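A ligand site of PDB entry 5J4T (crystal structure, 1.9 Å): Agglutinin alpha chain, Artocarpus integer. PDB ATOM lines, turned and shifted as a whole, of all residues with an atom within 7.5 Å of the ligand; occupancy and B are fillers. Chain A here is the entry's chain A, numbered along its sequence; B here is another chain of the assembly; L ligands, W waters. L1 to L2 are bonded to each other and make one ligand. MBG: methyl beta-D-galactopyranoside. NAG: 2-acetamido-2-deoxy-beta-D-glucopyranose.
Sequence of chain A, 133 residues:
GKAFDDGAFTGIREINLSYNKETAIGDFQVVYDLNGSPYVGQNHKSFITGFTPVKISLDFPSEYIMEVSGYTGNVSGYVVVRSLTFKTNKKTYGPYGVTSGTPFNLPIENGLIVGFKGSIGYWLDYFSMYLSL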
ATOM      1  N   GLY A   1      12.096   2.628  26.235  1.00  0.00           N
ATOM      2  CA  GLY A   1      10.636   2.384  26.449  1.00  0.00           C
ATOM      3  C   GLY A   1       9.928   1.642  25.317  1.00  0.00           C
ATOM      4  O   GLY A   1      10.493   1.458  24.240  1.00  0.00           O
ATOM      5  N   LYS A   2       8.720   1.160  25.576  1.00  0.00           N
ATOM      6  CA  LYS A   2       7.952   0.500  24.526  1.00  0.00           C
ATOM      7  C   LYS A   2       7.164   1.532  23.718  1.00  0.00           C
ATOM      8  O   LYS A   2       6.389   2.334  24.269  1.00  0.00           O
ATOM      9  CB  LYS A   2       6.993  -0.527  25.160  1.00  0.00           C
ATOM     10  CG  LYS A   2       6.168  -1.300  24.147  1.00  0.00           C
ATOM     11  CD  LYS A   2       5.054  -2.075  24.823  1.00  0.00           C
ATOM     12  CE  LYS A   2       4.769  -3.333  24.009  1.00  0.00           C
ATOM     13  NZ  LYS A   2       3.299  -3.585  23.862  1.00  0.00           N
ATOM     14  N   ALA A   3       7.338   1.490  22.389  1.00  0.00           N
ATOM     15  CA  ALA A   3       6.669   2.340  21.470  1.00  0.00           C
ATOM     16  C   ALA A   3       5.167   2.058  21.387  1.00  0.00           C
ATOM     17  O   ALA A   3       4.738   0.952  21.465  1.00  0.00           O
ATOM     18  CB  ALA A   3       7.286   2.178  20.096  1.00  0.00           C
ATOM     19  N   ILE A  25       5.276  11.586  33.927  1.00  0.00           N
ATOM     20  CA  ILE A  25       3.989  11.085  33.463  1.00  0.00           C
ATOM     21  C   ILE A  25       4.247   9.608  33.341  1.00  0.00           C
ATOM     22  O   ILE A  25       5.378   9.191  33.036  1.00  0.00           O
ATOM     23  CB  ILE A  25       3.570  11.686  32.076  1.00  0.00           C
ATOM     24  CG1 ILE A  25       3.206  13.197  32.156  1.00  0.00           C
ATOM     25  CG2 ILE A  25       2.452  10.842  31.400  1.00  0.00           C
ATOM     26  CD1 ILE A  25       2.066  13.634  33.074  1.00  0.00           C
ATOM     27  N   SER A  46       3.177   2.379  31.995  1.00  0.00           N
ATOM     28  CA  SER A  46       4.522   2.400  32.558  1.00  0.00           C
ATOM     29  C   SER A  46       4.989   0.990  32.977  1.00  0.00           C
ATOM     30  O   SER A  46       4.164   0.167  33.381  1.00  0.00           O
ATOM     31  CB  SER A  46       4.515   3.285  33.828  1.00  0.00           C
ATOM     32  OG  SER A  46       5.772   3.186  34.499  1.00  0.00           O
ATOM     33  N   PHE A  47       6.308   0.717  32.923  1.00  0.00           N
ATOM     34  CA  PHE A  47       6.887  -0.494  33.486  1.00  0.00           C
ATOM     35  C   PHE A  47       6.838  -0.495  35.039  1.00  0.00           C
ATOM     36  O   PHE A  47       7.106  -1.499  35.654  1.00  0.00           O
ATOM     37  CB  PHE A  47       8.339  -0.674  33.063  1.00  0.00           C
ATOM     38  CG  PHE A  47       8.571  -0.751  31.566  1.00  0.00           C
ATOM     39  CD1 PHE A  47       7.554  -1.052  30.668  1.00  0.00           C
ATOM     40  CD2 PHE A  47       9.865  -0.576  31.072  1.00  0.00           C
ATOM     41  CE1 PHE A  47       7.814  -1.130  29.281  1.00  0.00           C
ATOM     42  CE2 PHE A  47      10.151  -0.669  29.696  1.00  0.00           C
ATOM     43  CZ  PHE A  47       9.114  -0.945  28.806  1.00  0.00           C
ATOM     44  N   ILE A  48       6.432   0.603  35.686  1.00  0.00           N
ATOM     45  CA  ILE A  48       6.427   0.648  37.173  1.00  0.00           C
ATOM     46  C   ILE A  48       5.077   1.047  37.666  1.00  0.00           C
ATOM     47  O   ILE A  48       4.242   1.509  36.860  1.00  0.00           O
ATOM     48  CB  ILE A  48       7.561   1.535  37.813  1.00  0.00           C
ATOM     49  CG1 ILE A  48       7.298   3.054  37.617  1.00  0.00           C
ATOM     50  CG2 ILE A  48       8.937   1.079  37.275  1.00  0.00           C
ATOM     51  CD1 ILE A  48       8.433   3.984  38.060  1.00  0.00           C
ATOM     52  N   VAL A  75      14.817  12.330  34.512  1.00  0.00           N
ATOM     53  CA  VAL A  75      14.386  11.552  35.668  1.00  0.00           C
ATOM     54  C   VAL A  75      15.209  10.287  35.627  1.00  0.00           C
ATOM     55  O   VAL A  75      15.170   9.583  34.618  1.00  0.00           O
ATOM     56  CB  VAL A  75      12.864  11.239  35.619  1.00  0.00           C
ATOM     57  CG1 VAL A  75      12.499  10.381  36.834  1.00  0.00           C
ATOM     58  CG2 VAL A  75      12.057  12.542  35.584  1.00  0.00           C
ATOM     59  N   SER A  76      15.982  10.017  36.693  1.00  0.00           N
ATOM     60  CA  SER A  76      16.885   8.855  36.729  1.00  0.00           C
ATOM     61  C   SER A  76      17.838   8.844  35.530  1.00  0.00           C
ATOM     62  O   SER A  76      18.267   7.765  35.122  1.00  0.00           O
ATOM     63  CB  SER A  76      16.140   7.490  36.786  1.00  0.00           C
ATOM     64  OG  SER A  76      15.373   7.304  37.965  1.00  0.00           O
ATOM     65  N   GLY A  77      18.137  10.023  34.992  1.00  0.00           N
ATOM     66  CA  GLY A  77      19.032  10.235  33.877  1.00  0.00           C
ATOM     67  C   GLY A  77      18.397  10.006  32.529  1.00  0.00           C
ATOM     68  O   GLY A  77      19.074   9.980  31.549  1.00  0.00           O
ATOM     69  N   TYR A  78      17.097   9.795  32.483  1.00  0.00           N
ATOM     70  CA  TYR A  78      16.422   9.736  31.164  1.00  0.00           C
ATOM     71  C   TYR A  78      15.722  11.066  30.941  1.00  0.00           C
ATOM     72  O   TYR A  78      15.155  11.645  31.889  1.00  0.00           O
ATOM     73  CB  TYR A  78      15.419   8.592  31.108  1.00  0.00           C
ATOM     74  CG  TYR A  78      15.990   7.209  31.411  1.00  0.00           C
ATOM     75  CD1 TYR A  78      16.104   6.734  32.718  1.00  0.00           C
ATOM     76  CD2 TYR A  78      16.399   6.394  30.365  1.00  0.00           C
ATOM     77  CE1 TYR A  78      16.629   5.466  32.967  1.00  0.00           C
ATOM     78  CE2 TYR A  78      16.893   5.127  30.574  1.00  0.00           C
ATOM     79  CZ  TYR A  78      16.995   4.670  31.869  1.00  0.00           C
ATOM     80  OH  TYR A  78      17.526   3.384  32.020  1.00  0.00           O
ATOM     81  N   VAL A  79      15.764  11.576  29.717  1.00  0.00           N
ATOM     82  CA  VAL A  79      14.863  12.635  29.372  1.00  0.00           C
ATOM     83  C   VAL A  79      13.472  12.064  29.222  1.00  0.00           C
ATOM     84  O   VAL A  79      13.265  11.193  28.398  1.00  0.00           O
ATOM     85  CB  VAL A  79      15.235  13.319  28.037  1.00  0.00           C
ATOM     86  CG1 VAL A  79      14.247  14.453  27.775  1.00  0.00           C
ATOM     87  CG2 VAL A  79      16.690  13.809  28.055  1.00  0.00           C
ATOM     88  N   VAL A  80      12.484  12.641  29.937  1.00  0.00           N
ATOM     89  CA  VAL A  80      11.122  12.142  29.838  1.00  0.00           C
ATOM     90  C   VAL A  80      10.135  13.322  29.822  1.00  0.00           C
ATOM     91  O   VAL A  80      10.551  14.448  30.004  1.00  0.00           O
ATOM     92  CB  VAL A  80      10.799  11.093  30.955  1.00  0.00           C
ATOM     93  CG1 VAL A  80      11.708   9.849  30.849  1.00  0.00           C
ATOM     94  CG2 VAL A  80      10.938  11.684  32.339  1.00  0.00           C
ATOM     95  N   SER A 119       6.233   6.845  23.322  1.00  0.00           N
ATOM     96  CA  SER A 119       7.030   5.789  23.911  1.00  0.00           C
ATOM     97  C   SER A 119       7.021   5.833  25.459  1.00  0.00           C
ATOM     98  O   SER A 119       7.343   6.854  25.998  1.00  0.00           O
ATOM     99  CB  SER A 119       8.481   5.899  23.463  1.00  0.00           C
ATOM    100  OG  SER A 119       9.146   4.768  23.953  1.00  0.00           O
ATOM    101  N   ILE A 120       6.661   4.721  26.131  1.00  0.00           N
ATOM    102  CA  ILE A 120       6.627   4.679  27.629  1.00  0.00           C
ATOM    103  C   ILE A 120       7.528   3.579  28.181  1.00  0.00           C
ATOM    104  O   ILE A 120       7.392   2.394  27.778  1.00  0.00           O
ATOM    105  CB  ILE A 120       5.175   4.600  28.215  1.00  0.00           C
ATOM    106  CG1 ILE A 120       4.263   5.677  27.615  1.00  0.00           C
ATOM    107  CG2 ILE A 120       5.236   4.682  29.745  1.00  0.00           C
ATOM    108  CD1 ILE A 120       2.749   5.696  28.049  1.00  0.00           C
ATOM    109  N   GLY A 121       8.486   3.956  29.040  1.00  0.00           N
ATOM    110  CA  GLY A 121       9.243   2.990  29.851  1.00  0.00           C
ATOM    111  C   GLY A 121       8.831   3.051  31.294  1.00  0.00           C
ATOM    112  O   GLY A 121       7.692   2.657  31.650  1.00  0.00           O
ATOM    113  N   TYR A 122       9.712   3.534  32.161  1.00  0.00           N
ATOM    114  CA  TYR A 122       9.259   3.833  33.535  1.00  0.00           C
ATOM    115  C   TYR A 122       8.322   5.032  33.455  1.00  0.00           C
ATOM    116  O   TYR A 122       7.289   5.079  34.137  1.00  0.00           O
ATOM    117  CB  TYR A 122      10.439   4.171  34.394  1.00  0.00           C
ATOM    118  CG  TYR A 122      11.245   2.967  34.891  1.00  0.00           C
ATOM    119  CD1 TYR A 122      11.313   1.802  34.159  1.00  0.00           C
ATOM    120  CD2 TYR A 122      11.892   3.009  36.131  1.00  0.00           C
ATOM    121  CE1 TYR A 122      12.042   0.698  34.614  1.00  0.00           C
ATOM    122  CE2 TYR A 122      12.634   1.908  36.586  1.00  0.00           C
ATOM    123  CZ  TYR A 122      12.708   0.769  35.811  1.00  0.00           C
ATOM    124  OH  TYR A 122      13.450  -0.333  36.256  1.00  0.00           O
ATOM    125  N   TRP A 123       8.659   5.948  32.536  1.00  0.00           N
ATOM    126  CA  TRP A 123       7.854   7.138  32.283  1.00  0.00           C
ATOM    127  C   TRP A 123       7.619   7.296  30.796  1.00  0.00           C
ATOM    128  O   TRP A 123       8.231   6.571  30.007  1.00  0.00           O
ATOM    129  CB  TRP A 123       8.533   8.356  32.911  1.00  0.00           C
ATOM    130  CG  TRP A 123       8.853   8.084  34.370  1.00  0.00           C
ATOM    131  CD1 TRP A 123       7.973   8.069  35.439  1.00  0.00           C
ATOM    132  CD2 TRP A 123      10.155   7.660  34.929  1.00  0.00           C
ATOM    133  NE1 TRP A 123       8.635   7.681  36.613  1.00  0.00           N
ATOM    134  CE2 TRP A 123       9.941   7.446  36.352  1.00  0.00           C
ATOM    135  CE3 TRP A 123      11.415   7.439  34.395  1.00  0.00           C
ATOM    136  CZ2 TRP A 123      10.977   7.011  37.200  1.00  0.00           C
ATOM    137  CZ3 TRP A 123      12.459   7.059  35.257  1.00  0.00           C
ATOM    138  CH2 TRP A 123      12.230   6.834  36.621  1.00  0.00           C
ATOM    139  N   LEU A 124       6.678   8.187  30.422  1.00  0.00           N
ATOM    140  CA  LEU A 124       6.454   8.649  29.058  1.00  0.00           C
ATOM    141  C   LEU A 124       7.772   9.238  28.603  1.00  0.00           C
ATOM    142  O   LEU A 124       8.235  10.223  29.154  1.00  0.00           O
ATOM    143  CB  LEU A 124       5.423   9.774  29.050  1.00  0.00           C
ATOM    144  CG  LEU A 124       5.061  10.356  27.695  1.00  0.00           C
ATOM    145  CD1 LEU A 124       4.796   9.217  26.725  1.00  0.00           C
ATOM    146  CD2 LEU A 124       3.810  11.213  27.937  1.00  0.00           C
ATOM    147  N   ASP A 125       8.371   8.609  27.600  1.00  0.00           N
ATOM    148  CA  ASP A 125       9.677   9.054  27.072  1.00  0.00           C
ATOM    149  C   ASP A 125       9.505  10.248  26.119  1.00  0.00           C
ATOM    150  O   ASP A 125      10.168  11.277  26.247  1.00  0.00           O
ATOM    151  CB  ASP A 125      10.349   7.942  26.290  1.00  0.00           C
ATOM    152  CG  ASP A 125      10.598   6.709  27.125  1.00  0.00           C
ATOM    153  OD1 ASP A 125      11.152   6.858  28.224  1.00  0.00           O
ATOM    154  OD2 ASP A 125      10.220   5.601  26.648  1.00  0.00           O
ATOM    155  N   TYR A 126       8.624  10.089  25.140  1.00  0.00           N
ATOM    156  CA  TYR A 126       8.275  11.179  24.194  1.00  0.00           C
ATOM    157  C   TYR A 126       6.927  10.900  23.623  1.00  0.00           C
ATOM    158  O   TYR A 126       6.462   9.776  23.755  1.00  0.00           O
ATOM    159  CB  TYR A 126       9.310  11.233  23.056  1.00  0.00           C
ATOM    160  CG  TYR A 126       9.448   9.929  22.309  1.00  0.00           C
ATOM    161  CD1 TYR A 126       8.567   9.610  21.270  1.00  0.00           C
ATOM    162  CD2 TYR A 126      10.483   9.052  22.599  1.00  0.00           C
ATOM    163  CE1 TYR A 126       8.675   8.418  20.601  1.00  0.00           C
ATOM    164  CE2 TYR A 126      10.631   7.867  21.898  1.00  0.00           C
ATOM    165  CZ  TYR A 126       9.730   7.557  20.918  1.00  0.00           C
ATOM    166  OH  TYR A 126       9.845   6.357  20.230  1.00  0.00           O
ATOM    167  N   GLY B  15      10.143  15.219  24.139  1.00  0.00           N
ATOM    168  CA  GLY B  15      10.708  14.235  25.087  1.00  0.00           C
ATOM    169  C   GLY B  15      12.064  13.796  24.669  1.00  0.00           C
ATOM    170  O   GLY B  15      12.788  14.564  24.033  1.00  0.00           O
ATOM    171  N   ALA B  16      12.414  12.570  24.977  1.00  0.00           N
ATOM    172  CA  ALA B  16      13.686  12.072  24.619  1.00  0.00           C
ATOM    173  C   ALA B  16      13.925  12.047  23.105  1.00  0.00           C
ATOM    174  O   ALA B  16      13.029  11.719  22.278  1.00  0.00           O
ATOM    175  CB  ALA B  16      13.922  10.722  25.227  1.00  0.00           C
ATOM    176  N   LYS B  17      15.123  12.461  22.734  1.00  0.00           N
ATOM    177  CA  LYS B  17      15.487  12.457  21.315  1.00  0.00           C
ATOM    178  C   LYS B  17      16.210  11.190  20.915  1.00  0.00           C
ATOM    179  O   LYS B  17      15.569  10.182  20.612  1.00  0.00           O
ATOM    180  CB  LYS B  17      16.278  13.715  20.938  1.00  0.00           C
ATOM    181  CG  LYS B  17      15.357  14.908  20.717  1.00  0.00           C
ATOM    182  CD  LYS B  17      14.298  14.598  19.650  1.00  0.00           C
ATOM    183  CE  LYS B  17      12.964  15.297  19.914  1.00  0.00           C
ATOM    184  NZ  LYS B  17      12.235  14.785  21.114  1.00  0.00           N
HETATM  185  C1  MBG L   1      13.705   2.652  31.096  1.00  0.00           C
HETATM  186  C2  MBG L   1      13.730   2.286  29.589  1.00  0.00           C
HETATM  187  C3  MBG L   1      14.278   3.471  28.813  1.00  0.00           C
HETATM  188  C4  MBG L   1      13.390   4.725  29.088  1.00  0.00           C
HETATM  189  C5  MBG L   1      13.192   4.928  30.700  1.00  0.00           C
HETATM  190  C6  MBG L   1      12.369   6.198  31.032  1.00  0.00           C
HETATM  191  C7  MBG L   1      12.803   0.480  31.440  1.00  0.00           C
HETATM  192  O1  MBG L   1      13.719   1.463  31.991  1.00  0.00           O
HETATM  193  O2  MBG L   1      14.630   1.249  29.317  1.00  0.00           O
HETATM  194  O3  MBG L   1      14.254   3.150  27.413  1.00  0.00           O
HETATM  195  O4  MBG L   1      12.146   4.642  28.340  1.00  0.00           O
HETATM  196  O5  MBG L   1      12.643   3.687  31.322  1.00  0.00           O
HETATM  197  O6  MBG L   1      10.982   5.866  30.842  1.00  0.00           O
HETATM  198  C1  NAG L   2      15.417   3.680  26.796  1.00  0.00           C
HETATM  199  C2  NAG L   2      15.555   3.065  25.419  1.00  0.00           C
HETATM  200  C3  NAG L   2      16.647   3.854  24.661  1.00  0.00           C
HETATM  201  C4  NAG L   2      16.333   5.338  24.592  1.00  0.00           C
HETATM  202  C5  NAG L   2      16.175   5.864  26.001  1.00  0.00           C
HETATM  203  C6  NAG L   2      15.574   7.292  25.895  1.00  0.00           C
HETATM  204  C7  NAG L   2      15.077   0.685  25.759  1.00  0.00           C
HETATM  205  C8  NAG L   2      15.629  -0.735  25.795  1.00  0.00           C
HETATM  206  N2  NAG L   2      15.969   1.656  25.527  1.00  0.00           N
HETATM  207  O3  NAG L   2      16.812   3.404  23.313  1.00  0.00           O
HETATM  208  O4  NAG L   2      17.505   5.967  24.044  1.00  0.00           O
HETATM  209  O5  NAG L   2      15.132   5.085  26.616  1.00  0.00           O
HETATM  210  O6  NAG L   2      15.900   8.007  27.118  1.00  0.00           O
HETATM  211  O7  NAG L   2      13.886   0.910  25.938  1.00  0.00           O
HETATM  212  O   HOH W   1      17.141  10.179  27.403  1.00  0.00           O
HETATM  213  O   HOH W   2      13.525   8.189  28.035  1.00  0.00           O
HETATM  214  O   HOH W   3      18.093   1.556  27.408  1.00  0.00           O
HETATM  215  O   HOH W   4      12.186  -0.462  27.227  1.00  0.00           O
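The backbone NH (N) of Gly 121 is in hydrogen-bond range of the side-chain carboxylate (OD2) of Asp 125, at 3.4 Å. The backbone carbonyl oxygen (O) of Asp 125 lies within hydrogen-bond range of the backbone NH (N) of Ala 16 of chain B. The side-chain hydroxyl (OG) of Ser 46 is in hydrogen-bond range of the backbone carbonyl oxygen (O) of Tyr 122 (2.5 Å). The backbone NH (N) of Asp 125 sits at hydrogen-bond distance from the backbone carbonyl oxygen (O) of Ser 119. O of Gly 121 lies within hydrogen-bond range of N of Phe 47 (2.7 Å). OG of Ser 46 lies close to O of Gly 121 (3.5 Å).
Residues that only touch the ligand: Phe 47 (3.1 Å), Gly 121 (3.5 Å), Tyr 78 (3.5 Å), Val 80 (3.7 Å) and Ala 16 of chain B (3.9 Å). Hydrophobic or aromatic side chains that line the ligand: Phe 47, Tyr 78, Val 80, Tyr 122, Trp 123 and Ala 16 of chain B. Of the 24 residues printed, 9 come within 4 Å of the ligand.
The backbone carbonyl oxygen of Trp 123 sits at hydrogen-bond distance from an oxygen (O6) of MBG L1 (3.0 Å). O4 of MBG L1 is in hydrogen-bond range of OD1 of Asp 125 (2.4 Å). The backbone NH (N) of Gly 1 is in hydrogen-bond range of an oxygen (O7) of NAG L2, at 2.5 Å. An oxygen (O6) of MBG L1 lies within hydrogen-bond range of the backbone NH (N) of Tyr 122 (3.0 Å). An oxygen (O6) of MBG L1 is in hydrogen-bond range of the backbone NH (N) of Trp 123 (2.9 Å).
Water W1 bridges O6 of NAG L2 (2.5 Å) and N of Val 79 (3.0 Å). Water W4 lies within hydrogen-bond range of an oxygen (O7) of NAG L2 and the backbone NH (N) of Gly 1. Water W2 lies within hydrogen-bond range of an oxygen (O6) of NAG L2, the side-chain carboxylate (OD1) of Asp 125 and the backbone carbonyl oxygen (O) of Val 79.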
